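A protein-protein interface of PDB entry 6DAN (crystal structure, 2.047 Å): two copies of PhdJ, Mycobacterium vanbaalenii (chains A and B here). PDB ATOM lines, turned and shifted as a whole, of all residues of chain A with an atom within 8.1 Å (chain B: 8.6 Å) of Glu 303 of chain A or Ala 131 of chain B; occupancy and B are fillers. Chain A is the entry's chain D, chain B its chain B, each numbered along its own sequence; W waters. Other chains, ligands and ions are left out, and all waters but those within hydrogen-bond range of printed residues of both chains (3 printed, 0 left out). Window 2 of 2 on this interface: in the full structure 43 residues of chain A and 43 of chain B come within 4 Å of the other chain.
N of Ala 131 of chain B sits at hydrogen-bond distance from OD1 of Asp 129 of chain B, 3.3 Å away.
N of Gly 132 of chain B lies within hydrogen-bond range of OD1 of Asp 129 of chain B (2.8 Å).
OE1 of Gln 280 of chain A lies close to O of Tyr 277 of chain A, 3.3 Å away.
The backbone carbonyl oxygen (O) of Glu 303 of chain A lies within hydrogen-bond range of the side-chain amide nitrogen (NE2) of Gln 280 of chain A (2.9 Å).
O of Tyr 301 of chain A is in hydrogen-bond range of OG1 of Thr 297 of chain A.
Among the printed residues, pairs that only touch across the chains: Pro 300 of chain A with Leu 128 of chain B (3.4 Å), Thr 302 of chain A with Arg 135 of chain B (3.6 Å), Tyr 301 of chain A with Leu 128 of chain B (3.6 Å), Lys 276 of chain A with Leu 126 of chain B (3.6 Å), Glu 303 of chain A with Ala 131 of chain B (3.7 Å), Ile 279 of chain A with Leu 126 of chain B (3.8 Å), Glu 303 of chain A with Gly 132 of chain B (3.8 Å), Gln 280 of chain A with Leu 126 of chain B (3.8 Å), Lys 276 of chain A with Pro 127 of chain B (3.9 Å), Tyr 301 of chain A with Pro 127 of chain B (3.9 Å) and Glu 303 of chain A with Asp 129 of chain B (3.99 Å).
Water W3 lies within hydrogen-bond range of O of Lys 276 of chain A (2.7 Å), O of Pro 127 of chain B (2.7 Å) and NE2 of Gln 280 of chain A (3.1 Å).
Water W1 lies within hydrogen-bond range of the backbone carbonyl oxygen of Pro 300 of chain A (2.8 Å), the backbone carbonyl oxygen of Gly 132 of chain B (3.0 Å) and the backbone NH of Phe 136 of chain B (3.4 Å).
Water W2 bridges O of Glu 303 of chain A and N of Asp 129 of chain B.
No position is printed for both chains.
Printed residues of chain B within 4 Å of Ile 279 of chain A: Leu 126 (3.8 Å).
Ile 281 of chain A touches none of the printed residues of chain B.
Printed residues of chain B within 4 Å of Glu 303 of chain A: Asp 129 (3.99 Å), Ala 131 (3.7 Å), Gly 132 (3.8 Å) and Arg 135 (2.8 Å).
Glu 306 of chain A touches none of the printed residues of chain B.
Printed residues of chain A within 4 Å of Leu 126 of chain B: Lys 276 (3.6 Å), Ile 279 (3.8 Å), Gln 280 (3.8 Å) and Tyr 301 (2.6 Å).
Ala 131 of chain B touches just one residue of chain A: Glu 303.
Of the printed residues of chain A, Arg 135 of chain B touches Thr 302 (3.6 Å) and Glu 303 (2.8 Å).
The nearest printed residue of chain B that does not touch Tyr 301 of chain A is Gly 132 of chain B (6.8 Å).
The side-chain hydroxyl (OH) of Tyr 301 of chain A is in hydrogen-bond range of the backbone carbonyl oxygen (O) of Leu 126 of chain B, at 2.6 Å.
The side-chain carboxylate (OD2) of Asp 129 of chain B sits at hydrogen-bond distance from the side-chain hydroxyl (OH) of Tyr 277 of chain A.
The guanidinium group (NE) of Arg 135 of chain B is in salt-bridge range of the side-chain carboxylate (OE2) of Glu 303 of chain A (2.8 Å).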
ATOM      1  N   LYS A 276      23.853  -5.201 -13.825  1.00  0.00           N
ATOM      2  CA  LYS A 276      23.691  -6.480 -13.146  1.00  0.00           C
ATOM      3  C   LYS A 276      22.507  -6.466 -12.199  1.00  0.00           C
ATOM      4  O   LYS A 276      22.027  -7.534 -11.812  1.00  0.00           O
ATOM      5  CB  LYS A 276      24.962  -6.853 -12.366  1.00  0.00           C
ATOM      6  CG  LYS A 276      26.247  -6.663 -13.158  1.00  0.00           C
ATOM      7  CD  LYS A 276      27.455  -7.324 -12.475  1.00  0.00           C
ATOM      8  CE  LYS A 276      28.498  -7.737 -13.510  1.00  0.00           C
ATOM      9  NZ  LYS A 276      29.877  -7.301 -13.138  1.00  0.00           N
ATOM     10  N   TYR A 277      22.020  -5.279 -11.828  1.00  0.00           N
ATOM     11  CA  TYR A 277      20.982  -5.160 -10.812  1.00  0.00           C
ATOM     12  C   TYR A 277      19.918  -4.146 -11.209  1.00  0.00           C
ATOM     13  O   TYR A 277      19.295  -3.523 -10.338  1.00  0.00           O
ATOM     14  CB  TYR A 277      21.587  -4.759  -9.464  1.00  0.00           C
ATOM     15  CG  TYR A 277      22.559  -5.752  -8.879  1.00  0.00           C
ATOM     16  CD1 TYR A 277      22.109  -6.779  -8.060  1.00  0.00           C
ATOM     17  CD2 TYR A 277      23.927  -5.646  -9.117  1.00  0.00           C
ATOM     18  CE1 TYR A 277      22.990  -7.695  -7.497  1.00  0.00           C
ATOM     19  CE2 TYR A 277      24.823  -6.554  -8.560  1.00  0.00           C
ATOM     20  CZ  TYR A 277      24.341  -7.580  -7.743  1.00  0.00           C
ATOM     21  OH  TYR A 277      25.209  -8.492  -7.171  1.00  0.00           O
ATOM     22  N   ILE A 279      16.968  -4.328 -12.481  1.00  0.00           N
ATOM     23  CA  ILE A 279      15.606  -4.620 -12.048  1.00  0.00           C
ATOM     24  C   ILE A 279      15.426  -4.197 -10.597  1.00  0.00           C
ATOM     25  O   ILE A 279      14.469  -3.499 -10.248  1.00  0.00           O
ATOM     26  CB  ILE A 279      15.296  -6.115 -12.253  1.00  0.00           C
ATOM     27  CG1 ILE A 279      15.214  -6.445 -13.752  1.00  0.00           C
ATOM     28  CG2 ILE A 279      14.012  -6.528 -11.526  1.00  0.00           C
ATOM     29  CD1 ILE A 279      14.964  -7.916 -14.053  1.00  0.00           C
ATOM     30  N   GLN A 280      16.381  -4.578  -9.742  1.00  0.00           N
ATOM     31  CA  GLN A 280      16.302  -4.262  -8.323  1.00  0.00           C
ATOM     32  C   GLN A 280      16.461  -2.773  -8.069  1.00  0.00           C
ATOM     33  O   GLN A 280      15.725  -2.196  -7.262  1.00  0.00           O
ATOM     34  CB  GLN A 280      17.372  -5.039  -7.557  1.00  0.00           C
ATOM     35  CG  GLN A 280      17.292  -6.561  -7.688  1.00  0.00           C
ATOM     36  CD  GLN A 280      18.112  -7.135  -8.844  1.00  0.00           C
ATOM     37  OE1 GLN A 280      18.128  -6.596  -9.962  1.00  0.00           O
ATOM     38  NE2 GLN A 280      18.771  -8.256  -8.585  1.00  0.00           N
ATOM     39  N   ILE A 281      17.423  -2.135  -8.744  1.00  0.00           N
ATOM     40  CA  ILE A 281      17.694  -0.720  -8.508  1.00  0.00           C
ATOM     41  C   ILE A 281      16.548   0.133  -9.049  1.00  0.00           C
ATOM     42  O   ILE A 281      16.091   1.077  -8.392  1.00  0.00           O
ATOM     43  CB  ILE A 281      19.048  -0.326  -9.130  1.00  0.00           C
ATOM     44  CG1 ILE A 281      20.199  -1.111  -8.481  1.00  0.00           C
ATOM     45  CG2 ILE A 281      19.299   1.176  -9.026  1.00  0.00           C
ATOM     46  CD1 ILE A 281      21.576  -0.758  -9.028  1.00  0.00           C
ATOM     47  N   THR A 297      10.401  -6.993  -6.238  1.00  0.00           N
ATOM     48  CA  THR A 297      10.671  -7.586  -7.537  1.00  0.00           C
ATOM     49  C   THR A 297      10.350  -9.074  -7.518  1.00  0.00           C
ATOM     50  O   THR A 297      10.175  -9.684  -6.460  1.00  0.00           O
ATOM     51  CB  THR A 297      12.130  -7.361  -7.922  1.00  0.00           C
ATOM     52  OG1 THR A 297      12.978  -7.892  -6.894  1.00  0.00           O
ATOM     53  CG2 THR A 297      12.415  -5.865  -8.079  1.00  0.00           C
ATOM     54  N   ARG A 298      10.291  -9.673  -8.716  1.00  0.00           N
ATOM     55  CA  ARG A 298       9.921 -11.075  -8.806  1.00  0.00           C
ATOM     56  C   ARG A 298      11.150 -11.964  -8.691  1.00  0.00           C
ATOM     57  O   ARG A 298      12.267 -11.548  -9.020  1.00  0.00           O
ATOM     58  CB  ARG A 298       9.219 -11.363 -10.132  1.00  0.00           C
ATOM     59  CG  ARG A 298       7.717 -11.033 -10.162  1.00  0.00           C
ATOM     60  CD  ARG A 298       7.492  -9.556 -10.564  1.00  0.00           C
ATOM     61  NE  ARG A 298       6.071  -9.226 -10.575  1.00  0.00           N
ATOM     62  CZ  ARG A 298       5.573  -8.068 -10.995  1.00  0.00           C
ATOM     63  NH1 ARG A 298       6.391  -7.129 -11.446  1.00  0.00           N
ATOM     64  NH2 ARG A 298       4.253  -7.855 -10.965  1.00  0.00           N
ATOM     65  N   PRO A 299      10.972 -13.206  -8.245  1.00  0.00           N
ATOM     66  CA  PRO A 299      12.085 -14.169  -8.265  1.00  0.00           C
ATOM     67  C   PRO A 299      12.570 -14.373  -9.688  1.00  0.00           C
ATOM     68  O   PRO A 299      11.755 -14.469 -10.617  1.00  0.00           O
ATOM     69  CB  PRO A 299      11.458 -15.455  -7.695  1.00  0.00           C
ATOM     70  CG  PRO A 299      10.275 -14.977  -6.908  1.00  0.00           C
ATOM     71  CD  PRO A 299       9.740 -13.799  -7.700  1.00  0.00           C
ATOM     72  N   PRO A 300      13.886 -14.479  -9.905  1.00  0.00           N
ATOM     73  CA  PRO A 300      14.973 -14.653  -8.941  1.00  0.00           C
ATOM     74  C   PRO A 300      15.718 -13.389  -8.556  1.00  0.00           C
ATOM     75  O   PRO A 300      16.736 -13.493  -7.860  1.00  0.00           O
ATOM     76  CB  PRO A 300      15.918 -15.567  -9.703  1.00  0.00           C
ATOM     77  CG  PRO A 300      15.851 -14.980 -11.083  1.00  0.00           C
ATOM     78  CD  PRO A 300      14.386 -14.607 -11.282  1.00  0.00           C
ATOM     79  N   TYR A 301      15.259 -12.228  -9.028  1.00  0.00           N
ATOM     80  CA  TYR A 301      16.044 -10.993  -8.955  1.00  0.00           C
ATOM     81  C   TYR A 301      15.634 -10.157  -7.739  1.00  0.00           C
ATOM     82  O   TYR A 301      15.174  -9.017  -7.841  1.00  0.00           O
ATOM     83  CB  TYR A 301      15.903 -10.214 -10.260  1.00  0.00           C
ATOM     84  CG  TYR A 301      16.460 -10.984 -11.449  1.00  0.00           C
ATOM     85  CD1 TYR A 301      17.791 -11.363 -11.477  1.00  0.00           C
ATOM     86  CD2 TYR A 301      15.665 -11.337 -12.522  1.00  0.00           C
ATOM     87  CE1 TYR A 301      18.323 -12.066 -12.548  1.00  0.00           C
ATOM     88  CE2 TYR A 301      16.191 -12.048 -13.607  1.00  0.00           C
ATOM     89  CZ  TYR A 301      17.522 -12.410 -13.607  1.00  0.00           C
ATOM     90  OH  TYR A 301      18.080 -13.112 -14.661  1.00  0.00           O
ATOM     91  N   THR A 302      15.818 -10.759  -6.564  1.00  0.00           N
ATOM     92  CA  THR A 302      15.496 -10.125  -5.295  1.00  0.00           C
ATOM     93  C   THR A 302      16.723  -9.854  -4.446  1.00  0.00           C
ATOM     94  O   THR A 302      16.589  -9.329  -3.335  1.00  0.00           O
ATOM     95  CB  THR A 302      14.529 -10.991  -4.485  1.00  0.00           C
ATOM     96  OG1 THR A 302      15.184 -12.214  -4.115  1.00  0.00           O
ATOM     97  CG2 THR A 302      13.271 -11.289  -5.292  1.00  0.00           C
ATOM     98  N   GLU A 303      17.907 -10.194  -4.931  1.00  0.00           N
ATOM     99  CA  GLU A 303      19.145 -10.027  -4.183  1.00  0.00           C
ATOM    100  C   GLU A 303      19.973  -8.920  -4.825  1.00  0.00           C
ATOM    101  O   GLU A 303      20.119  -8.883  -6.053  1.00  0.00           O
ATOM    102  CB  GLU A 303      19.920 -11.347  -4.151  1.00  0.00           C
ATOM    103  CG  GLU A 303      19.173 -12.460  -3.412  1.00  0.00           C
ATOM    104  CD  GLU A 303      19.181 -12.262  -1.907  1.00  0.00           C
ATOM    105  OE1 GLU A 303      20.004 -11.464  -1.413  1.00  0.00           O
ATOM    106  OE2 GLU A 303      18.368 -12.904  -1.212  1.00  0.00           O
ATOM    107  N   VAL A 304      20.518  -8.033  -3.996  1.00  0.00           N
ATOM    108  CA  VAL A 304      21.212  -6.838  -4.480  1.00  0.00           C
ATOM    109  C   VAL A 304      21.937  -6.182  -3.308  1.00  0.00           C
ATOM    110  O   VAL A 304      21.375  -6.103  -2.201  1.00  0.00           O
ATOM    111  CB  VAL A 304      20.224  -5.861  -5.155  1.00  0.00           C
ATOM    112  CG1 VAL A 304      18.980  -5.645  -4.286  1.00  0.00           C
ATOM    113  CG2 VAL A 304      20.887  -4.543  -5.443  1.00  0.00           C
ATOM    114  N   PRO A 305      23.182  -5.736  -3.481  1.00  0.00           N
ATOM    115  CA  PRO A 305      23.814  -4.923  -2.439  1.00  0.00           C
ATOM    116  C   PRO A 305      22.895  -3.777  -2.036  1.00  0.00           C
ATOM    117  O   PRO A 305      22.393  -3.034  -2.883  1.00  0.00           O
ATOM    118  CB  PRO A 305      25.103  -4.424  -3.106  1.00  0.00           C
ATOM    119  CG  PRO A 305      25.421  -5.482  -4.128  1.00  0.00           C
ATOM    120  CD  PRO A 305      24.092  -6.006  -4.612  1.00  0.00           C
ATOM    121  N   GLU A 306      22.645  -3.662  -0.731  1.00  0.00           N
ATOM    122  CA  GLU A 306      21.658  -2.704  -0.241  1.00  0.00           C
ATOM    123  C   GLU A 306      22.002  -1.285  -0.666  1.00  0.00           C
ATOM    124  O   GLU A 306      21.109  -0.483  -0.971  1.00  0.00           O
ATOM    125  CB  GLU A 306      21.558  -2.794   1.281  1.00  0.00           C
ATOM    126  CG  GLU A 306      20.684  -3.922   1.807  1.00  0.00           C
ATOM    127  CD  GLU A 306      21.320  -5.311   1.707  1.00  0.00           C
ATOM    128  OE1 GLU A 306      22.560  -5.446   1.560  1.00  0.00           O
ATOM    129  OE2 GLU A 306      20.552  -6.286   1.787  1.00  0.00           O
ATOM    130  N   TYR A 308      23.231  -0.214  -3.348  1.00  0.00           N
ATOM    131  CA  TYR A 308      22.757   0.093  -4.693  1.00  0.00           C
ATOM    132  C   TYR A 308      21.295   0.533  -4.670  1.00  0.00           C
ATOM    133  O   TYR A 308      20.869   1.306  -5.536  1.00  0.00           O
ATOM    134  CB  TYR A 308      22.912  -1.106  -5.629  1.00  0.00           C
ATOM    135  CG  TYR A 308      24.315  -1.656  -5.851  1.00  0.00           C
ATOM    136  CD1 TYR A 308      25.418  -1.174  -5.150  1.00  0.00           C
ATOM    137  CD2 TYR A 308      24.527  -2.680  -6.779  1.00  0.00           C
ATOM    138  CE1 TYR A 308      26.693  -1.704  -5.366  1.00  0.00           C
ATOM    139  CE2 TYR A 308      25.783  -3.209  -7.001  1.00  0.00           C
ATOM    140  CZ  TYR A 308      26.857  -2.723  -6.299  1.00  0.00           C
ATOM    141  OH  TYR A 308      28.093  -3.255  -6.550  1.00  0.00           O
ATOM    142  N   LEU A 309      20.515   0.035  -3.705  1.00  0.00           N
ATOM    143  CA  LEU A 309      19.123   0.460  -3.569  1.00  0.00           C
ATOM    144  C   LEU A 309      19.031   1.897  -3.082  1.00  0.00           C
ATOM    145  O   LEU A 309      18.149   2.646  -3.523  1.00  0.00           O
ATOM    146  CB  LEU A 309      18.375  -0.461  -2.609  1.00  0.00           C
ATOM    147  CG  LEU A 309      18.279  -1.925  -3.023  1.00  0.00           C
ATOM    148  CD1 LEU A 309      17.500  -2.731  -1.990  1.00  0.00           C
ATOM    149  CD2 LEU A 309      17.640  -2.027  -4.410  1.00  0.00           C
ATOM    150  N   LEU B 126      19.328 -11.096 -16.470  1.00  0.00           N
ATOM    151  CA  LEU B 126      20.346 -10.481 -15.639  1.00  0.00           C
ATOM    152  C   LEU B 126      21.181 -11.582 -14.981  1.00  0.00           C
ATOM    153  O   LEU B 126      20.675 -12.684 -14.728  1.00  0.00           O
ATOM    154  CB  LEU B 126      19.742  -9.592 -14.545  1.00  0.00           C
ATOM    155  CG  LEU B 126      19.421  -8.120 -14.879  1.00  0.00           C
ATOM    156  CD1 LEU B 126      18.398  -8.025 -15.984  1.00  0.00           C
ATOM    157  CD2 LEU B 126      18.930  -7.375 -13.643  1.00  0.00           C
ATOM    158  N   PRO B 127      22.459 -11.335 -14.715  1.00  0.00           N
ATOM    159  CA  PRO B 127      23.230 -12.312 -13.940  1.00  0.00           C
ATOM    160  C   PRO B 127      22.714 -12.353 -12.515  1.00  0.00           C
ATOM    161  O   PRO B 127      22.138 -11.387 -12.000  1.00  0.00           O
ATOM    162  CB  PRO B 127      24.670 -11.775 -14.004  1.00  0.00           C
ATOM    163  CG  PRO B 127      24.491 -10.284 -14.210  1.00  0.00           C
ATOM    164  CD  PRO B 127      23.240 -10.128 -15.046  1.00  0.00           C
ATOM    165  N   LEU B 128      22.891 -13.499 -11.884  1.00  0.00           N
ATOM    166  CA  LEU B 128      22.596 -13.662 -10.474  1.00  0.00           C
ATOM    167  C   LEU B 128      23.925 -13.700  -9.735  1.00  0.00           C
ATOM    168  O   LEU B 128      24.867 -14.352 -10.193  1.00  0.00           O
ATOM    169  CB  LEU B 128      21.787 -14.942 -10.238  1.00  0.00           C
ATOM    170  CG  LEU B 128      20.324 -14.957 -10.707  1.00  0.00           C
ATOM    171  CD1 LEU B 128      19.753 -16.387 -10.816  1.00  0.00           C
ATOM    172  CD2 LEU B 128      19.433 -14.071  -9.797  1.00  0.00           C
ATOM    173  N   ASP B 129      24.021 -12.982  -8.621  1.00  0.00           N
ATOM    174  CA  ASP B 129      25.207 -13.095  -7.783  1.00  0.00           C
ATOM    175  C   ASP B 129      25.085 -14.377  -6.945  1.00  0.00           C
ATOM    176  O   ASP B 129      24.162 -15.177  -7.118  1.00  0.00           O
ATOM    177  CB  ASP B 129      25.402 -11.823  -6.954  1.00  0.00           C
ATOM    178  CG  ASP B 129      24.209 -11.489  -6.068  1.00  0.00           C
ATOM    179  OD1 ASP B 129      23.463 -12.402  -5.662  1.00  0.00           O
ATOM    180  OD2 ASP B 129      24.036 -10.292  -5.751  1.00  0.00           O
ATOM    181  N   ASP B 130      26.015 -14.592  -6.017  1.00  0.00           N
ATOM    182  CA  ASP B 130      26.013 -15.842  -5.266  1.00  0.00           C
ATOM    183  C   ASP B 130      24.765 -15.960  -4.403  1.00  0.00           C
ATOM    184  O   ASP B 130      24.141 -17.024  -4.352  1.00  0.00           O
ATOM    185  CB  ASP B 130      27.292 -15.952  -4.431  1.00  0.00           C
ATOM    186  CG  ASP B 130      28.472 -16.483  -5.241  1.00  0.00           C
ATOM    187  OD1 ASP B 130      28.264 -16.899  -6.403  1.00  0.00           O
ATOM    188  OD2 ASP B 130      29.604 -16.500  -4.724  1.00  0.00           O
ATOM    189  N   ALA B 131      24.362 -14.871  -3.742  1.00  0.00           N
ATOM    190  CA  ALA B 131      23.129 -14.929  -2.961  1.00  0.00           C
ATOM    191  C   ALA B 131      21.932 -15.241  -3.853  1.00  0.00           C
ATOM    192  O   ALA B 131      21.065 -16.048  -3.484  1.00  0.00           O
ATOM    193  CB  ALA B 131      22.914 -13.618  -2.203  1.00  0.00           C
ATOM    194  N   GLY B 132      21.868 -14.615  -5.037  1.00  0.00           N
ATOM    195  CA  GLY B 132      20.780 -14.907  -5.960  1.00  0.00           C
ATOM    196  C   GLY B 132      20.800 -16.343  -6.454  1.00  0.00           C
ATOM    197  O   GLY B 132      19.748 -16.961  -6.649  1.00  0.00           O
ATOM    198  N   ILE B 133      21.997 -16.894  -6.663  1.00  0.00           N
ATOM    199  CA  ILE B 133      22.102 -18.263  -7.156  1.00  0.00           C
ATOM    200  C   ILE B 133      21.623 -19.250  -6.097  1.00  0.00           C
ATOM    201  O   ILE B 133      20.860 -20.178  -6.392  1.00  0.00           O
ATOM    202  CB  ILE B 133      23.543 -18.569  -7.596  1.00  0.00           C
ATOM    203  CG1 ILE B 133      23.892 -17.811  -8.882  1.00  0.00           C
ATOM    204  CG2 ILE B 133      23.750 -20.104  -7.756  1.00  0.00           C
ATOM    205  CD1 ILE B 133      25.382 -17.802  -9.162  1.00  0.00           C
ATOM    206  N   VAL B 134      22.050 -19.056  -4.846  1.00  0.00           N
ATOM    207  CA  VAL B 134      21.654 -19.981  -3.781  1.00  0.00           C
ATOM    208  C   VAL B 134      20.149 -19.914  -3.551  1.00  0.00           C
ATOM    209  O   VAL B 134      19.496 -20.941  -3.307  1.00  0.00           O
ATOM    210  CB  VAL B 134      22.439 -19.693  -2.482  1.00  0.00           C
ATOM    211  CG1 VAL B 134      21.833 -20.424  -1.297  1.00  0.00           C
ATOM    212  CG2 VAL B 134      23.915 -20.064  -2.638  1.00  0.00           C
ATOM    213  N   ARG B 135      19.575 -18.706  -3.606  1.00  0.00           N
ATOM    214  CA  ARG B 135      18.145 -18.569  -3.340  1.00  0.00           C
ATOM    215  C   ARG B 135      17.318 -19.274  -4.411  1.00  0.00           C
ATOM    216  O   ARG B 135      16.316 -19.932  -4.097  1.00  0.00           O
ATOM    217  CB  ARG B 135      17.756 -17.095  -3.248  1.00  0.00           C
ATOM    218  CG  ARG B 135      16.266 -16.894  -3.051  1.00  0.00           C
ATOM    219  CD  ARG B 135      15.934 -15.436  -2.793  1.00  0.00           C
ATOM    220  NE  ARG B 135      16.469 -14.956  -1.518  1.00  0.00           N
ATOM    221  CZ  ARG B 135      15.852 -15.116  -0.352  1.00  0.00           C
ATOM    222  NH1 ARG B 135      14.693 -15.754  -0.303  1.00  0.00           N
ATOM    223  NH2 ARG B 135      16.392 -14.638   0.763  1.00  0.00           N
ATOM    224  N   PHE B 136      17.756 -19.182  -5.670  1.00  0.00           N
ATOM    225  CA  PHE B 136      17.072 -19.844  -6.780  1.00  0.00           C
ATOM    226  C   PHE B 136      17.037 -21.357  -6.591  1.00  0.00           C
ATOM    227  O   PHE B 136      15.966 -21.979  -6.617  1.00  0.00           O
ATOM    228  CB  PHE B 136      17.774 -19.477  -8.093  1.00  0.00           C
ATOM    229  CG  PHE B 136      17.381 -20.334  -9.271  1.00  0.00           C
ATOM    230  CD1 PHE B 136      16.146 -20.160  -9.896  1.00  0.00           C
ATOM    231  CD2 PHE B 136      18.268 -21.275  -9.786  1.00  0.00           C
ATOM    232  CE1 PHE B 136      15.789 -20.929 -11.001  1.00  0.00           C
ATOM    233  CE2 PHE B 136      17.926 -22.059 -10.885  1.00  0.00           C
ATOM    234  CZ  PHE B 136      16.679 -21.889 -11.492  1.00  0.00           C
ATOM    235  N   TYR B 137      18.207 -21.971  -6.412  1.00  0.00           N
ATOM    236  CA  TYR B 137      18.259 -23.421  -6.281  1.00  0.00           C
ATOM    237  C   TYR B 137      17.481 -23.892  -5.060  1.00  0.00           C
ATOM    238  O   TYR B 137      16.783 -24.907  -5.123  1.00  0.00           O
ATOM    239  CB  TYR B 137      19.713 -23.882  -6.226  1.00  0.00           C
ATOM    240  CG  TYR B 137      20.320 -23.947  -7.612  1.00  0.00           C
ATOM    241  CD1 TYR B 137      19.839 -24.846  -8.554  1.00  0.00           C
ATOM    242  CD2 TYR B 137      21.337 -23.077  -7.992  1.00  0.00           C
ATOM    243  CE1 TYR B 137      20.377 -24.907  -9.832  1.00  0.00           C
ATOM    244  CE2 TYR B 137      21.884 -23.133  -9.270  1.00  0.00           C
ATOM    245  CZ  TYR B 137      21.399 -24.048 -10.182  1.00  0.00           C
ATOM    246  OH  TYR B 137      21.930 -24.097 -11.454  1.00  0.00           O
ATOM    247  N   ARG B 138      17.582 -23.160  -3.947  1.00  0.00           N
ATOM    248  CA  ARG B 138      16.806 -23.498  -2.761  1.00  0.00           C
ATOM    249  C   ARG B 138      15.309 -23.373  -3.031  1.00  0.00           C
ATOM    250  O   ARG B 138      14.519 -24.216  -2.587  1.00  0.00           O
ATOM    251  CB  ARG B 138      17.219 -22.600  -1.592  1.00  0.00           C
ATOM    252  CG  ARG B 138      16.379 -22.842  -0.348  1.00  0.00           C
ATOM    253  CD  ARG B 138      16.841 -21.997   0.836  1.00  0.00           C
ATOM    254  NE  ARG B 138      15.764 -21.694   1.795  1.00  0.00           N
ATOM    255  CZ  ARG B 138      14.583 -21.143   1.493  1.00  0.00           C
ATOM    256  NH1 ARG B 138      14.274 -20.808   0.249  1.00  0.00           N
ATOM    257  NH2 ARG B 138      13.686 -20.935   2.443  1.00  0.00           N
ATOM    258  N   ASP B 139      14.901 -22.326  -3.757  1.00  0.00           N
ATOM    259  CA  ASP B 139      13.508 -22.202  -4.172  1.00  0.00           C
ATOM    260  C   ASP B 139      13.070 -23.433  -4.951  1.00  0.00           C
ATOM    261  O   ASP B 139      12.021 -24.023  -4.664  1.00  0.00           O
ATOM    262  CB  ASP B 139      13.299 -20.947  -5.031  1.00  0.00           C
ATOM    263  CG  ASP B 139      13.356 -19.640  -4.227  1.00  0.00           C
ATOM    264  OD1 ASP B 139      13.470 -19.678  -2.979  1.00  0.00           O
ATOM    265  OD2 ASP B 139      13.283 -18.554  -4.860  1.00  0.00           O
ATOM    266  N   GLY B 163      30.219 -19.203  -7.297  1.00  0.00           N
ATOM    267  CA  GLY B 163      31.302 -18.984  -6.347  1.00  0.00           C
ATOM    268  C   GLY B 163      31.431 -20.108  -5.333  1.00  0.00           C
ATOM    269  O   GLY B 163      30.475 -20.830  -5.024  1.00  0.00           O
ATOM    270  N   PRO B 165      31.588 -19.863  -2.081  1.00  0.00           N
ATOM    271  CA  PRO B 165      30.569 -19.748  -1.019  1.00  0.00           C
ATOM    272  C   PRO B 165      29.196 -20.216  -1.457  1.00  0.00           C
ATOM    273  O   PRO B 165      28.437 -20.739  -0.631  1.00  0.00           O
ATOM    274  CB  PRO B 165      30.567 -18.247  -0.688  1.00  0.00           C
ATOM    275  CG  PRO B 165      31.886 -17.743  -1.204  1.00  0.00           C
ATOM    276  CD  PRO B 165      32.138 -18.538  -2.437  1.00  0.00           C
ATOM    277  N   ALA B 166      28.844 -20.034  -2.730  1.00  0.00           N
ATOM    278  CA  ALA B 166      27.567 -20.560  -3.196  1.00  0.00           C
ATOM    279  C   ALA B 166      27.563 -22.084  -3.189  1.00  0.00           C
ATOM    280  O   ALA B 166      26.542 -22.704  -2.867  1.00  0.00           O
ATOM    281  CB  ALA B 166      27.251 -20.025  -4.589  1.00  0.00           C
ATOM    282  N   ALA B 169      26.829 -23.410   0.243  1.00  0.00           N
ATOM    283  CA  ALA B 169      25.403 -23.359   0.565  1.00  0.00           C
ATOM    284  C   ALA B 169      24.616 -24.400  -0.221  1.00  0.00           C
ATOM    285  O   ALA B 169      23.700 -25.033   0.316  1.00  0.00           O
ATOM    286  CB  ALA B 169      24.849 -21.967   0.291  1.00  0.00           C
ATOM    287  N   LEU B 170      24.943 -24.578  -1.503  1.00  0.00           N
ATOM    288  CA  LEU B 170      24.243 -25.563  -2.316  1.00  0.00           C
ATOM    289  C   LEU B 170      24.379 -26.967  -1.735  1.00  0.00           C
ATOM    290  O   LEU B 170      23.448 -27.781  -1.838  1.00  0.00           O
ATOM    291  CB  LEU B 170      24.781 -25.527  -3.750  1.00  0.00           C
ATOM    292  CG  LEU B 170      24.413 -24.285  -4.571  1.00  0.00           C
ATOM    293  CD1 LEU B 170      25.067 -24.330  -5.952  1.00  0.00           C
ATOM    294  CD2 LEU B 170      22.899 -24.141  -4.691  1.00  0.00           C
HETATM  295  O   HOH W   1      16.905 -15.976  -6.531  1.00  0.00           O
HETATM  296  O   HOH W   2      21.430 -10.942  -8.206  1.00  0.00           O
HETATM  297  O   HOH W   3      20.978  -9.530 -10.374  1.00  0.00           O
